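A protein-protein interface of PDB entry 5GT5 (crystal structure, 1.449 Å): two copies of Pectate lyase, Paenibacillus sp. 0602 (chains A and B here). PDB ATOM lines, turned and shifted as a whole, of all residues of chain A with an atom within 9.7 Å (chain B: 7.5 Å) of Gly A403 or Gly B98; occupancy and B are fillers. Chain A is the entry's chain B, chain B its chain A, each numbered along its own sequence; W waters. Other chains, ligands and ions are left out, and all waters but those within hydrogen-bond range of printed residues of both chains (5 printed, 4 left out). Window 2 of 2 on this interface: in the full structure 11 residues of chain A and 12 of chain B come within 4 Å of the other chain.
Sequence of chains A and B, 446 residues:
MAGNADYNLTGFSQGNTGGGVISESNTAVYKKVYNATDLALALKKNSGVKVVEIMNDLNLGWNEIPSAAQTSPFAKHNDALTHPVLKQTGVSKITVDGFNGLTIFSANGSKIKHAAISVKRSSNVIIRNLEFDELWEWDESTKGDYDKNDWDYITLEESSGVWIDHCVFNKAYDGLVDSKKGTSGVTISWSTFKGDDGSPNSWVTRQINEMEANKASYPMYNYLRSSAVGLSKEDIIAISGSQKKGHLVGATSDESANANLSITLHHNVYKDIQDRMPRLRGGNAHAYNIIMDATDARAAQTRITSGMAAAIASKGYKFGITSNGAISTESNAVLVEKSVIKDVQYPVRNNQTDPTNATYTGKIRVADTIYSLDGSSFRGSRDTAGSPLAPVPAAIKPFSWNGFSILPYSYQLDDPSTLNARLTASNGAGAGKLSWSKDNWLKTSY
No position is printed for both chains. Of the 7 pairs that touch across the chains among the printed residues, none has its exchanged pair printed and touching as well.
The side-chain amino group of Lys B50 is in hydrogen-bond range of the backbone carbonyl oxygen of Asn B100, at 2.8 Å. N of Gly B98 lies within hydrogen-bond range of O of Lys B120, 3.1 Å away. The backbone NH (N) of Gly B98 sits close to the backbone carbonyl oxygen (O) of Arg B121 (3.3 Å). N of Gly B98 is in hydrogen-bond range of OG of Ser B122 (3.3 Å). The backbone carbonyl oxygen (O) of Phe B99 lies within hydrogen-bond range of the backbone NH (N) of Ser B123. N of Gly B101 lies within hydrogen-bond range of O of Ser B123 (2.9 Å).
OD1 of Asn B46 sits close to N of Phe A404 (3.2 Å). N of Gly A403 lies close to O of Gly B98 (3.5 Å). The side-chain amide nitrogen of Asn B100 is in hydrogen-bond range of the backbone carbonyl oxygen of Ala A259 (3.1 Å).
Among the printed residues, pairs that only touch across the chains: Ala A259 with Ser B123, Gly A403 with Asn B46, Ser A405 with Asn B46 and Asn A260 with Asn B100.
Of the 20 printed residues of chain A, 5 touch a printed residue of chain B. Printed residues of chain A that touch a printed residue of chain B: Ala A259, Asn A260, Gly A403, Phe A404 and Ser A405. Among the printed residues, 7 pairs touch across the chains.
Water W2 bridges O of Arg B121 (2.8 Å) and OD1 of Asn A402 (2.9 Å). Water W4 bridges the backbone carbonyl oxygen of Gly A403 (2.8 Å) and the backbone NH of Gly B48 (3.0 Å). Water W5 bridges O of Asn B46 (2.8 Å) and N of Ser A405 (3.0 Å). Water W1 lies within hydrogen-bond range of ND2 of Asn B100 and OD1 of Asn A260. Water W3 lies within hydrogen-bond range of the backbone carbonyl oxygen (O) of Asn B100, the side-chain amino group (NZ) of Lys B50 and the backbone carbonyl oxygen (O) of Gly A403.
Printed residues of chain B within 4 Å of Gly A403: Asn B46 and Gly B98. Of the printed residues of chain B, Phe A404 touches Asn B46. Ile A406 touches none of the printed residues of chain B. Pro A408 touches none of the printed residues of chain B. Asn B46 touches just these residues of chain A: Gly A403 (3.5 Å), Phe A404 (3.2 Å) and Ser A405 (3.5 Å). No residue of chain A comes within 4 Å of Asp B97. Of chain A, only Gly A403 (3.4 Å) comes within 4 Å of Gly B98. Of the printed residues of chain A, Asn B100 touches Ala A259 and Asn A260. The nearest residue of chain A that does not touch Gly B98 is Asn A402 (4.5 Å). The nearest printed residue of chain A that does not touch Ser B123 is Gly A282 (6.0 Å).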
ATOM      1  N   PHE A  12     -26.209  17.346 -15.972  1.00  0.00           N
ATOM      2  CA  PHE A  12     -25.392  18.307 -15.233  1.00  0.00           C
ATOM      3  C   PHE A  12     -24.804  19.396 -16.118  1.00  0.00           C
ATOM      4  O   PHE A  12     -24.473  20.462 -15.621  1.00  0.00           O
ATOM      5  CB  PHE A  12     -24.283  17.601 -14.442  1.00  0.00           C
ATOM      6  CG  PHE A  12     -24.774  16.914 -13.181  1.00  0.00           C
ATOM      7  CD1 PHE A  12     -25.227  17.683 -12.115  1.00  0.00           C
ATOM      8  CD2 PHE A  12     -24.737  15.536 -13.041  1.00  0.00           C
ATOM      9  CE1 PHE A  12     -25.679  17.063 -10.948  1.00  0.00           C
ATOM     10  CE2 PHE A  12     -25.181  14.913 -11.873  1.00  0.00           C
ATOM     11  CZ  PHE A  12     -25.644  15.681 -10.830  1.00  0.00           C
ATOM     12  N   ALA A 259     -15.364  15.836  -4.726  1.00  0.00           N
ATOM     13  CA  ALA A 259     -16.736  16.046  -4.331  1.00  0.00           C
ATOM     14  C   ALA A 259     -17.449  16.981  -5.301  1.00  0.00           C
ATOM     15  O   ALA A 259     -18.692  16.944  -5.422  1.00  0.00           O
ATOM     16  CB  ALA A 259     -16.796  16.612  -2.927  1.00  0.00           C
ATOM     17  N   ASN A 260     -16.669  17.756  -6.049  1.00  0.00           N
ATOM     18  CA  ASN A 260     -17.238  18.680  -7.026  1.00  0.00           C
ATOM     19  C   ASN A 260     -17.508  18.063  -8.385  1.00  0.00           C
ATOM     20  O   ASN A 260     -18.136  18.697  -9.228  1.00  0.00           O
ATOM     21  CB  ASN A 260     -16.327  19.886  -7.238  1.00  0.00           C
ATOM     22  CG  ASN A 260     -16.111  20.679  -5.980  1.00  0.00           C
ATOM     23  OD1 ASN A 260     -17.039  20.884  -5.195  1.00  0.00           O
ATOM     24  ND2 ASN A 260     -14.884  21.154  -5.792  1.00  0.00           N
ATOM     25  N   LEU A 261     -17.029  16.847  -8.603  1.00  0.00           N
ATOM     26  CA  LEU A 261     -17.316  16.159  -9.878  1.00  0.00           C
ATOM     27  C   LEU A 261     -18.801  15.900 -10.016  1.00  0.00           C
ATOM     28  O   LEU A 261     -19.451  15.370  -9.104  1.00  0.00           O
ATOM     29  CB  LEU A 261     -16.563  14.825  -9.943  1.00  0.00           C
ATOM     30  CG  LEU A 261     -15.048  14.959  -9.877  1.00  0.00           C
ATOM     31  CD1 LEU A 261     -14.462  13.647  -9.409  1.00  0.00           C
ATOM     32  CD2 LEU A 261     -14.455  15.406 -11.214  1.00  0.00           C
ATOM     33  N   GLY A 282     -16.075  10.306  -4.894  1.00  0.00           N
ATOM     34  CA  GLY A 282     -16.472  11.523  -4.179  1.00  0.00           C
ATOM     35  C   GLY A 282     -17.665  12.320  -4.663  1.00  0.00           C
ATOM     36  O   GLY A 282     -18.411  12.842  -3.845  1.00  0.00           O
ATOM     37  N   GLY A 283     -17.839  12.434  -5.974  1.00  0.00           N
ATOM     38  CA  GLY A 283     -18.848  13.361  -6.499  1.00  0.00           C
ATOM     39  C   GLY A 283     -20.219  12.751  -6.708  1.00  0.00           C
ATOM     40  O   GLY A 283     -20.688  11.941  -5.919  1.00  0.00           O
ATOM     41  N   ASN A 284     -20.880  13.169  -7.780  1.00  0.00           N
ATOM     42  CA  ASN A 284     -22.239  12.723  -8.135  1.00  0.00           C
ATOM     43  C   ASN A 284     -22.264  12.295  -9.589  1.00  0.00           C
ATOM     44  O   ASN A 284     -21.908  13.086 -10.459  1.00  0.00           O
ATOM     45  CB  ASN A 284     -23.254  13.877  -7.927  1.00  0.00           C
ATOM     46  CG  ASN A 284     -23.409  14.252  -6.481  1.00  0.00           C
ATOM     47  OD1 ASN A 284     -23.907  13.448  -5.700  1.00  0.00           O
ATOM     48  ND2 ASN A 284     -22.991  15.465  -6.112  1.00  0.00           N
ATOM     49  N   SER A 331     -17.121   7.790  -0.887  1.00  0.00           N
ATOM     50  CA  SER A 331     -18.278   8.614  -0.529  1.00  0.00           C
ATOM     51  C   SER A 331     -18.976   9.258  -1.708  1.00  0.00           C
ATOM     52  O   SER A 331     -19.826  10.103  -1.521  1.00  0.00           O
ATOM     53  CB  SER A 331     -17.914   9.652   0.528  1.00  0.00           C
ATOM     54  OG  SER A 331     -17.406   9.000   1.699  1.00  0.00           O
ATOM     55  N   ASN A 332     -18.651   8.827  -2.916  1.00  0.00           N
ATOM     56  CA  ASN A 332     -19.365   9.257  -4.116  1.00  0.00           C
ATOM     57  C   ASN A 332     -20.806   8.750  -4.144  1.00  0.00           C
ATOM     58  O   ASN A 332     -21.168   7.850  -3.378  1.00  0.00           O
ATOM     59  CB  ASN A 332     -18.630   8.622  -5.260  1.00  0.00           C
ATOM     60  N   ALA A 333     -21.598   9.291  -5.067  1.00  0.00           N
ATOM     61  CA  ALA A 333     -22.977   8.848  -5.262  1.00  0.00           C
ATOM     62  C   ALA A 333     -23.183   8.517  -6.726  1.00  0.00           C
ATOM     63  O   ALA A 333     -23.006   9.401  -7.574  1.00  0.00           O
ATOM     64  CB  ALA A 333     -23.941   9.964  -4.855  1.00  0.00           C
ATOM     65  N   LYS A 363     -21.508   5.345  -2.347  1.00  0.00           N
ATOM     66  CA  LYS A 363     -22.935   5.047  -2.377  1.00  0.00           C
ATOM     67  C   LYS A 363     -23.392   4.801  -3.802  1.00  0.00           C
ATOM     68  O   LYS A 363     -23.013   5.544  -4.707  1.00  0.00           O
ATOM     69  CB  LYS A 363     -23.717   6.254  -1.818  1.00  0.00           C
ATOM     70  CG  LYS A 363     -23.335   6.626  -0.373  1.00  0.00           C
ATOM     71  CD  LYS A 363     -23.979   7.944   0.066  1.00  0.00           C
ATOM     72  CE  LYS A 363     -23.332   9.168  -0.569  1.00  0.00           C
ATOM     73  NZ  LYS A 363     -24.003  10.416  -0.091  1.00  0.00           N
ATOM     74  N   SER A 400     -27.665   8.213  -1.123  1.00  0.00           N
ATOM     75  CA  SER A 400     -28.198   9.569  -1.195  1.00  0.00           C
ATOM     76  C   SER A 400     -27.209  10.364  -2.022  1.00  0.00           C
ATOM     77  O   SER A 400     -26.011  10.009  -2.117  1.00  0.00           O
ATOM     78  CB  SER A 400     -28.308  10.185   0.200  1.00  0.00           C
ATOM     79  OG  SER A 400     -27.016  10.436   0.733  1.00  0.00           O
ATOM     80  N   TRP A 401     -27.694  11.434  -2.649  1.00  0.00           N
ATOM     81  CA  TRP A 401     -26.792  12.315  -3.388  1.00  0.00           C
ATOM     82  C   TRP A 401     -25.875  13.093  -2.466  1.00  0.00           C
ATOM     83  O   TRP A 401     -26.138  13.205  -1.265  1.00  0.00           O
ATOM     84  CB  TRP A 401     -27.588  13.264  -4.258  1.00  0.00           C
ATOM     85  CG  TRP A 401     -28.368  12.540  -5.348  1.00  0.00           C
ATOM     86  CD1 TRP A 401     -29.735  12.357  -5.414  1.00  0.00           C
ATOM     87  CD2 TRP A 401     -27.825  11.896  -6.513  1.00  0.00           C
ATOM     88  NE1 TRP A 401     -30.059  11.643  -6.549  1.00  0.00           N
ATOM     89  CE2 TRP A 401     -28.910  11.351  -7.243  1.00  0.00           C
ATOM     90  CE3 TRP A 401     -26.536  11.744  -7.022  1.00  0.00           C
ATOM     91  CZ2 TRP A 401     -28.728  10.657  -8.442  1.00  0.00           C
ATOM     92  CZ3 TRP A 401     -26.358  11.039  -8.197  1.00  0.00           C
ATOM     93  CH2 TRP A 401     -27.435  10.512  -8.892  1.00  0.00           C
ATOM     94  N   ASN A 402     -24.816  13.664  -3.035  1.00  0.00           N
ATOM     95  CA  ASN A 402     -23.933  14.484  -2.228  1.00  0.00           C
ATOM     96  C   ASN A 402     -24.242  15.967  -2.400  1.00  0.00           C
ATOM     97  O   ASN A 402     -23.762  16.611  -3.337  1.00  0.00           O
ATOM     98  CB  ASN A 402     -22.479  14.195  -2.580  1.00  0.00           C
ATOM     99  CG  ASN A 402     -22.047  12.842  -2.112  1.00  0.00           C
ATOM    100  OD1 ASN A 402     -22.364  12.432  -0.996  1.00  0.00           O
ATOM    101  ND2 ASN A 402     -21.348  12.097  -2.986  1.00  0.00           N
ATOM    102  N   GLY A 403     -24.971  16.504  -1.420  1.00  0.00           N
ATOM    103  CA  GLY A 403     -25.232  17.931  -1.328  1.00  0.00           C
ATOM    104  C   GLY A 403     -26.611  18.417  -1.674  1.00  0.00           C
ATOM    105  O   GLY A 403     -26.965  19.578  -1.422  1.00  0.00           O
ATOM    106  N   PHE A 404     -27.419  17.523  -2.212  1.00  0.00           N
ATOM    107  CA  PHE A 404     -28.791  17.861  -2.572  1.00  0.00           C
ATOM    108  C   PHE A 404     -29.652  16.625  -2.369  1.00  0.00           C
ATOM    109  O   PHE A 404     -29.143  15.494  -2.371  1.00  0.00           O
ATOM    110  CB  PHE A 404     -28.889  18.417  -4.010  1.00  0.00           C
ATOM    111  CG  PHE A 404     -28.116  17.614  -5.036  1.00  0.00           C
ATOM    112  CD1 PHE A 404     -28.641  16.431  -5.567  1.00  0.00           C
ATOM    113  CD2 PHE A 404     -26.881  18.078  -5.502  1.00  0.00           C
ATOM    114  CE1 PHE A 404     -27.948  15.711  -6.515  1.00  0.00           C
ATOM    115  CE2 PHE A 404     -26.175  17.348  -6.459  1.00  0.00           C
ATOM    116  CZ  PHE A 404     -26.712  16.163  -6.962  1.00  0.00           C
ATOM    117  N   SER A 405     -30.961  16.843  -2.236  1.00  0.00           N
ATOM    118  CA  SER A 405     -31.874  15.749  -2.022  1.00  0.00           C
ATOM    119  C   SER A 405     -32.241  15.063  -3.336  1.00  0.00           C
ATOM    120  O   SER A 405     -32.195  13.838  -3.440  1.00  0.00           O
ATOM    121  CB  SER A 405     -33.163  16.272  -1.387  1.00  0.00           C
ATOM    122  OG  SER A 405     -34.049  15.193  -1.221  1.00  0.00           O
ATOM    123  N   ILE A 406     -32.608  15.848  -4.341  1.00  0.00           N
ATOM    124  CA  ILE A 406     -32.928  15.300  -5.658  1.00  0.00           C
ATOM    125  C   ILE A 406     -32.100  15.988  -6.718  1.00  0.00           C
ATOM    126  O   ILE A 406     -31.642  17.103  -6.525  1.00  0.00           O
ATOM    127  CB  ILE A 406     -34.421  15.379  -5.989  1.00  0.00           C
ATOM    128  CG1 ILE A 406     -34.876  16.813  -6.043  1.00  0.00           C
ATOM    129  CG2 ILE A 406     -35.243  14.600  -4.980  1.00  0.00           C
ATOM    130  CD1 ILE A 406     -36.265  16.955  -6.717  1.00  0.00           C
ATOM    131  N   LEU A 407     -31.905  15.319  -7.856  1.00  0.00           N
ATOM    132  CA  LEU A 407     -31.085  15.889  -8.911  1.00  0.00           C
ATOM    133  C   LEU A 407     -31.619  17.232  -9.359  1.00  0.00           C
ATOM    134  O   LEU A 407     -32.836  17.430  -9.422  1.00  0.00           O
ATOM    135  CB  LEU A 407     -31.069  14.945 -10.117  1.00  0.00           C
ATOM    136  CG  LEU A 407     -30.237  13.677  -9.920  1.00  0.00           C
ATOM    137  CD1 LEU A 407     -30.678  12.690 -10.979  1.00  0.00           C
ATOM    138  CD2 LEU A 407     -28.737  13.971 -10.062  1.00  0.00           C
ATOM    139  N   PRO A 408     -30.716  18.172  -9.655  1.00  0.00           N
ATOM    140  CA  PRO A 408     -31.084  19.560  -9.989  1.00  0.00           C
ATOM    141  C   PRO A 408     -31.528  19.763 -11.439  1.00  0.00           C
ATOM    142  O   PRO A 408     -31.413  20.856 -11.980  1.00  0.00           O
ATOM    143  CB  PRO A 408     -29.799  20.339  -9.688  1.00  0.00           C
ATOM    144  CG  PRO A 408     -28.731  19.355  -9.984  1.00  0.00           C
ATOM    145  CD  PRO A 408     -29.255  18.010  -9.536  1.00  0.00           C
ATOM    146  N   LYS B  45     -29.963  19.612   6.735  1.00  0.00           N
ATOM    147  CA  LYS B  45     -29.451  18.752   5.660  1.00  0.00           C
ATOM    148  C   LYS B  45     -30.190  19.034   4.352  1.00  0.00           C
ATOM    149  O   LYS B  45     -31.419  19.178   4.321  1.00  0.00           O
ATOM    150  CB  LYS B  45     -29.591  17.275   6.065  1.00  0.00           C
ATOM    151  CG  LYS B  45     -29.042  16.288   5.056  1.00  0.00           C
ATOM    152  CD  LYS B  45     -29.235  14.861   5.594  1.00  0.00           C
ATOM    153  CE  LYS B  45     -28.887  13.820   4.528  1.00  0.00           C
ATOM    154  NZ  LYS B  45     -29.271  12.438   4.959  1.00  0.00           N
ATOM    155  N   ASN B  46     -29.403  19.161   3.275  1.00  0.00           N
ATOM    156  CA  ASN B  46     -29.914  19.436   1.937  1.00  0.00           C
ATOM    157  C   ASN B  46     -30.550  20.784   1.743  1.00  0.00           C
ATOM    158  O   ASN B  46     -31.320  20.987   0.794  1.00  0.00           O
ATOM    159  CB  ASN B  46     -30.773  18.276   1.411  1.00  0.00           C
ATOM    160  CG  ASN B  46     -29.960  17.042   1.148  1.00  0.00           C
ATOM    161  OD1 ASN B  46     -28.844  17.147   0.654  1.00  0.00           O
ATOM    162  ND2 ASN B  46     -30.510  15.876   1.452  1.00  0.00           N
ATOM    163  N   SER B  47     -30.198  21.735   2.603  1.00  0.00           N
ATOM    164  CA  SER B  47     -30.715  23.084   2.437  1.00  0.00           C
ATOM    165  C   SER B  47     -30.157  23.732   1.172  1.00  0.00           C
ATOM    166  O   SER B  47     -30.758  24.699   0.646  1.00  0.00           O
ATOM    167  CB  SER B  47     -30.337  23.944   3.640  1.00  0.00           C
ATOM    168  OG  SER B  47     -28.954  24.269   3.600  1.00  0.00           O
ATOM    169  N   GLY B  48     -28.982  23.272   0.740  1.00  0.00           N
ATOM    170  CA  GLY B  48     -28.303  23.852  -0.421  1.00  0.00           C
ATOM    171  C   GLY B  48     -27.597  25.173  -0.167  1.00  0.00           C
ATOM    172  O   GLY B  48     -27.036  25.800  -1.089  1.00  0.00           O
ATOM    173  N   VAL B  49     -27.604  25.601   1.089  1.00  0.00           N
ATOM    174  CA  VAL B  49     -26.996  26.882   1.426  1.00  0.00           C
ATOM    175  C   VAL B  49     -25.494  26.789   1.251  1.00  0.00           C
ATOM    176  O   VAL B  49     -24.896  25.768   1.620  1.00  0.00           O
ATOM    177  CB  VAL B  49     -27.380  27.280   2.856  1.00  0.00           C
ATOM    178  CG1 VAL B  49     -26.541  28.441   3.371  1.00  0.00           C
ATOM    179  CG2 VAL B  49     -28.841  27.633   2.902  1.00  0.00           C
ATOM    180  N   LYS B  50     -24.891  27.818   0.657  1.00  0.00           N
ATOM    181  CA  LYS B  50     -23.463  27.880   0.373  1.00  0.00           C
ATOM    182  C   LYS B  50     -22.682  28.726   1.358  1.00  0.00           C
ATOM    183  O   LYS B  50     -21.549  28.352   1.691  1.00  0.00           O
ATOM    184  CB  LYS B  50     -23.257  28.434  -1.043  1.00  0.00           C
ATOM    185  CG  LYS B  50     -23.823  27.542  -2.144  1.00  0.00           C
ATOM    186  CD  LYS B  50     -22.830  26.383  -2.315  1.00  0.00           C
ATOM    187  CE  LYS B  50     -23.421  25.104  -2.797  1.00  0.00           C
ATOM    188  NZ  LYS B  50     -22.292  24.094  -2.838  1.00  0.00           N
ATOM    189  N   THR B  95     -25.517  19.367  14.061  1.00  0.00           N
ATOM    190  CA  THR B  95     -24.886  18.453  13.114  1.00  0.00           C
ATOM    191  C   THR B  95     -25.045  18.938  11.680  1.00  0.00           C
ATOM    192  O   THR B  95     -26.170  18.943  11.146  1.00  0.00           O
ATOM    193  CB  THR B  95     -25.447  17.025  13.234  1.00  0.00           C
ATOM    194  OG1 THR B  95     -25.200  16.545  14.559  1.00  0.00           O
ATOM    195  CG2 THR B  95     -24.737  16.090  12.267  1.00  0.00           C
ATOM    196  N   VAL B  96     -23.918  19.296  11.068  1.00  0.00           N
ATOM    197  CA  VAL B  96     -23.837  19.695   9.674  1.00  0.00           C
ATOM    198  C   VAL B  96     -23.572  18.437   8.888  1.00  0.00           C
ATOM    199  O   VAL B  96     -22.461  17.875   8.973  1.00  0.00           O
ATOM    200  CB  VAL B  96     -22.661  20.682   9.503  1.00  0.00           C
ATOM    201  CG1 VAL B  96     -22.446  21.076   8.063  1.00  0.00           C
ATOM    202  CG2 VAL B  96     -22.897  21.950  10.358  1.00  0.00           C
ATOM    203  N   ASP B  97     -24.579  17.981   8.134  1.00  0.00           N
ATOM    204  CA  ASP B  97     -24.576  16.639   7.550  1.00  0.00           C
ATOM    205  C   ASP B  97     -24.794  16.711   6.042  1.00  0.00           C
ATOM    206  O   ASP B  97     -25.744  17.335   5.564  1.00  0.00           O
ATOM    207  CB  ASP B  97     -25.715  15.815   8.183  1.00  0.00           C
ATOM    208  CG  ASP B  97     -25.667  14.329   7.834  1.00  0.00           C
ATOM    209  OD1 ASP B  97     -24.838  13.892   7.012  1.00  0.00           O
ATOM    210  OD2 ASP B  97     -26.493  13.585   8.404  1.00  0.00           O
ATOM    211  N   GLY B  98     -23.876  16.140   5.282  1.00  0.00           N
ATOM    212  CA  GLY B  98     -24.118  15.988   3.860  1.00  0.00           C
ATOM    213  C   GLY B  98     -23.909  17.234   3.025  1.00  0.00           C
ATOM    214  O   GLY B  98     -24.423  17.310   1.906  1.00  0.00           O
ATOM    215  N   PHE B  99     -23.173  18.227   3.520  1.00  0.00           N
ATOM    216  CA  PHE B  99     -22.899  19.438   2.766  1.00  0.00           C
ATOM    217  C   PHE B  99     -21.724  19.270   1.816  1.00  0.00           C
ATOM    218  O   PHE B  99     -20.781  18.536   2.127  1.00  0.00           O
ATOM    219  CB  PHE B  99     -22.682  20.629   3.715  1.00  0.00           C
ATOM    220  CG  PHE B  99     -23.974  21.215   4.206  1.00  0.00           C
ATOM    221  CD1 PHE B  99     -24.645  20.620   5.273  1.00  0.00           C
ATOM    222  CD2 PHE B  99     -24.569  22.298   3.558  1.00  0.00           C
ATOM    223  CE1 PHE B  99     -25.908  21.121   5.699  1.00  0.00           C
ATOM    224  CE2 PHE B  99     -25.820  22.797   3.976  1.00  0.00           C
ATOM    225  CZ  PHE B  99     -26.473  22.217   5.077  1.00  0.00           C
ATOM    226  N   ASN B 100     -21.812  19.875   0.635  1.00  0.00           N
ATOM    227  CA  ASN B 100     -20.678  19.960  -0.271  1.00  0.00           C
ATOM    228  C   ASN B 100     -20.446  21.385  -0.711  1.00  0.00           C
ATOM    229  O   ASN B 100     -21.179  21.933  -1.545  1.00  0.00           O
ATOM    230  CB  ASN B 100     -20.835  19.108  -1.513  1.00  0.00           C
ATOM    231  CG  ASN B 100     -19.601  19.199  -2.415  1.00  0.00           C
ATOM    232  OD1 ASN B 100     -18.478  19.296  -1.945  1.00  0.00           O
ATOM    233  ND2 ASN B 100     -19.835  19.304  -3.712  1.00  0.00           N
ATOM    234  N   GLY B 101     -19.457  22.013  -0.109  1.00  0.00           N
ATOM    235  CA  GLY B 101     -19.112  23.363  -0.468  1.00  0.00           C
ATOM    236  C   GLY B 101     -19.905  24.330   0.372  1.00  0.00           C
ATOM    237  O   GLY B 101     -20.955  24.820  -0.043  1.00  0.00           O
ATOM    238  N   VAL B 119     -19.494  17.991  12.185  1.00  0.00           N
ATOM    239  CA  VAL B 119     -19.522  17.970  10.725  1.00  0.00           C
ATOM    240  C   VAL B 119     -19.416  16.533  10.290  1.00  0.00           C
ATOM    241  O   VAL B 119     -18.439  15.845  10.602  1.00  0.00           O
ATOM    242  CB  VAL B 119     -18.388  18.792  10.118  1.00  0.00           C
ATOM    243  CG1 VAL B 119     -18.425  18.712   8.579  1.00  0.00           C
ATOM    244  CG2 VAL B 119     -18.440  20.265  10.605  1.00  0.00           C
ATOM    245  N   LYS B 120     -20.443  16.030   9.617  1.00  0.00           N
ATOM    246  CA  LYS B 120     -20.471  14.616   9.203  1.00  0.00           C
ATOM    247  C   LYS B 120     -20.734  14.521   7.730  1.00  0.00           C
ATOM    248  O   LYS B 120     -21.554  15.260   7.200  1.00  0.00           O
ATOM    249  CB  LYS B 120     -21.604  13.840   9.893  1.00  0.00           C
ATOM    250  CG  LYS B 120     -21.427  13.716  11.393  1.00  0.00           C
ATOM    251  CD  LYS B 120     -22.562  12.920  12.022  1.00  0.00           C
ATOM    252  CE  LYS B 120     -22.358  12.728  13.535  1.00  0.00           C
ATOM    253  NZ  LYS B 120     -23.473  11.903  14.094  1.00  0.00           N
ATOM    254  N   ARG B 121     -20.033  13.600   7.090  1.00  0.00           N
ATOM    255  CA  ARG B 121     -20.343  13.234   5.692  1.00  0.00           C
ATOM    256  C   ARG B 121     -20.387  14.477   4.795  1.00  0.00           C
ATOM    257  O   ARG B 121     -21.249  14.597   3.918  1.00  0.00           O
ATOM    258  CB  ARG B 121     -21.656  12.447   5.628  1.00  0.00           C
ATOM    259  CG  ARG B 121     -21.602  11.078   6.286  1.00  0.00           C
ATOM    260  CD  ARG B 121     -22.996  10.450   6.392  1.00  0.00           C
ATOM    261  NE  ARG B 121     -23.870  11.100   7.371  1.00  0.00           N
ATOM    262  CZ  ARG B 121     -24.025  10.712   8.638  1.00  0.00           C
ATOM    263  NH1 ARG B 121     -23.335   9.678   9.116  1.00  0.00           N
ATOM    264  NH2 ARG B 121     -24.861  11.377   9.432  1.00  0.00           N
ATOM    265  N   SER B 122     -19.472  15.418   5.025  1.00  0.00           N
ATOM    266  CA  SER B 122     -19.456  16.674   4.281  1.00  0.00           C
ATOM    267  C   SER B 122     -18.117  16.881   3.591  1.00  0.00           C
ATOM    268  O   SER B 122     -17.087  16.272   3.938  1.00  0.00           O
ATOM    269  CB  SER B 122     -19.739  17.827   5.234  1.00  0.00           C
ATOM    270  OG  SER B 122     -21.084  17.770   5.725  1.00  0.00           O
ATOM    271  N   SER B 123     -18.110  17.749   2.589  1.00  0.00           N
ATOM    272  CA  SER B 123     -16.887  18.055   1.863  1.00  0.00           C
ATOM    273  C   SER B 123     -16.802  19.536   1.613  1.00  0.00           C
ATOM    274  O   SER B 123     -17.824  20.233   1.457  1.00  0.00           O
ATOM    275  CB  SER B 123     -16.828  17.299   0.542  1.00  0.00           C
ATOM    276  OG  SER B 123     -18.010  17.548  -0.195  1.00  0.00           O
ATOM    277  N   SER B 159     -15.472  13.104   6.692  1.00  0.00           N
ATOM    278  CA  SER B 159     -15.526  14.309   5.860  1.00  0.00           C
ATOM    279  C   SER B 159     -14.213  14.494   5.092  1.00  0.00           C
ATOM    280  O   SER B 159     -13.214  13.781   5.330  1.00  0.00           O
ATOM    281  CB  SER B 159     -15.858  15.526   6.728  1.00  0.00           C
ATOM    282  OG  SER B 159     -17.211  15.427   7.208  1.00  0.00           O
HETATM  283  O   HOH W   1     -20.122  21.451  -5.909  1.00  0.00           O
HETATM  284  O   HOH W   2     -22.490  13.660   1.648  1.00  0.00           O
HETATM  285  O   HOH W   3     -24.292  21.309  -2.838  1.00  0.00           O
HETATM  286  O   HOH W   4     -27.001  21.077   0.902  1.00  0.00           O
HETATM  287  O   HOH W   5     -31.452  19.779  -1.775  1.00  0.00           O
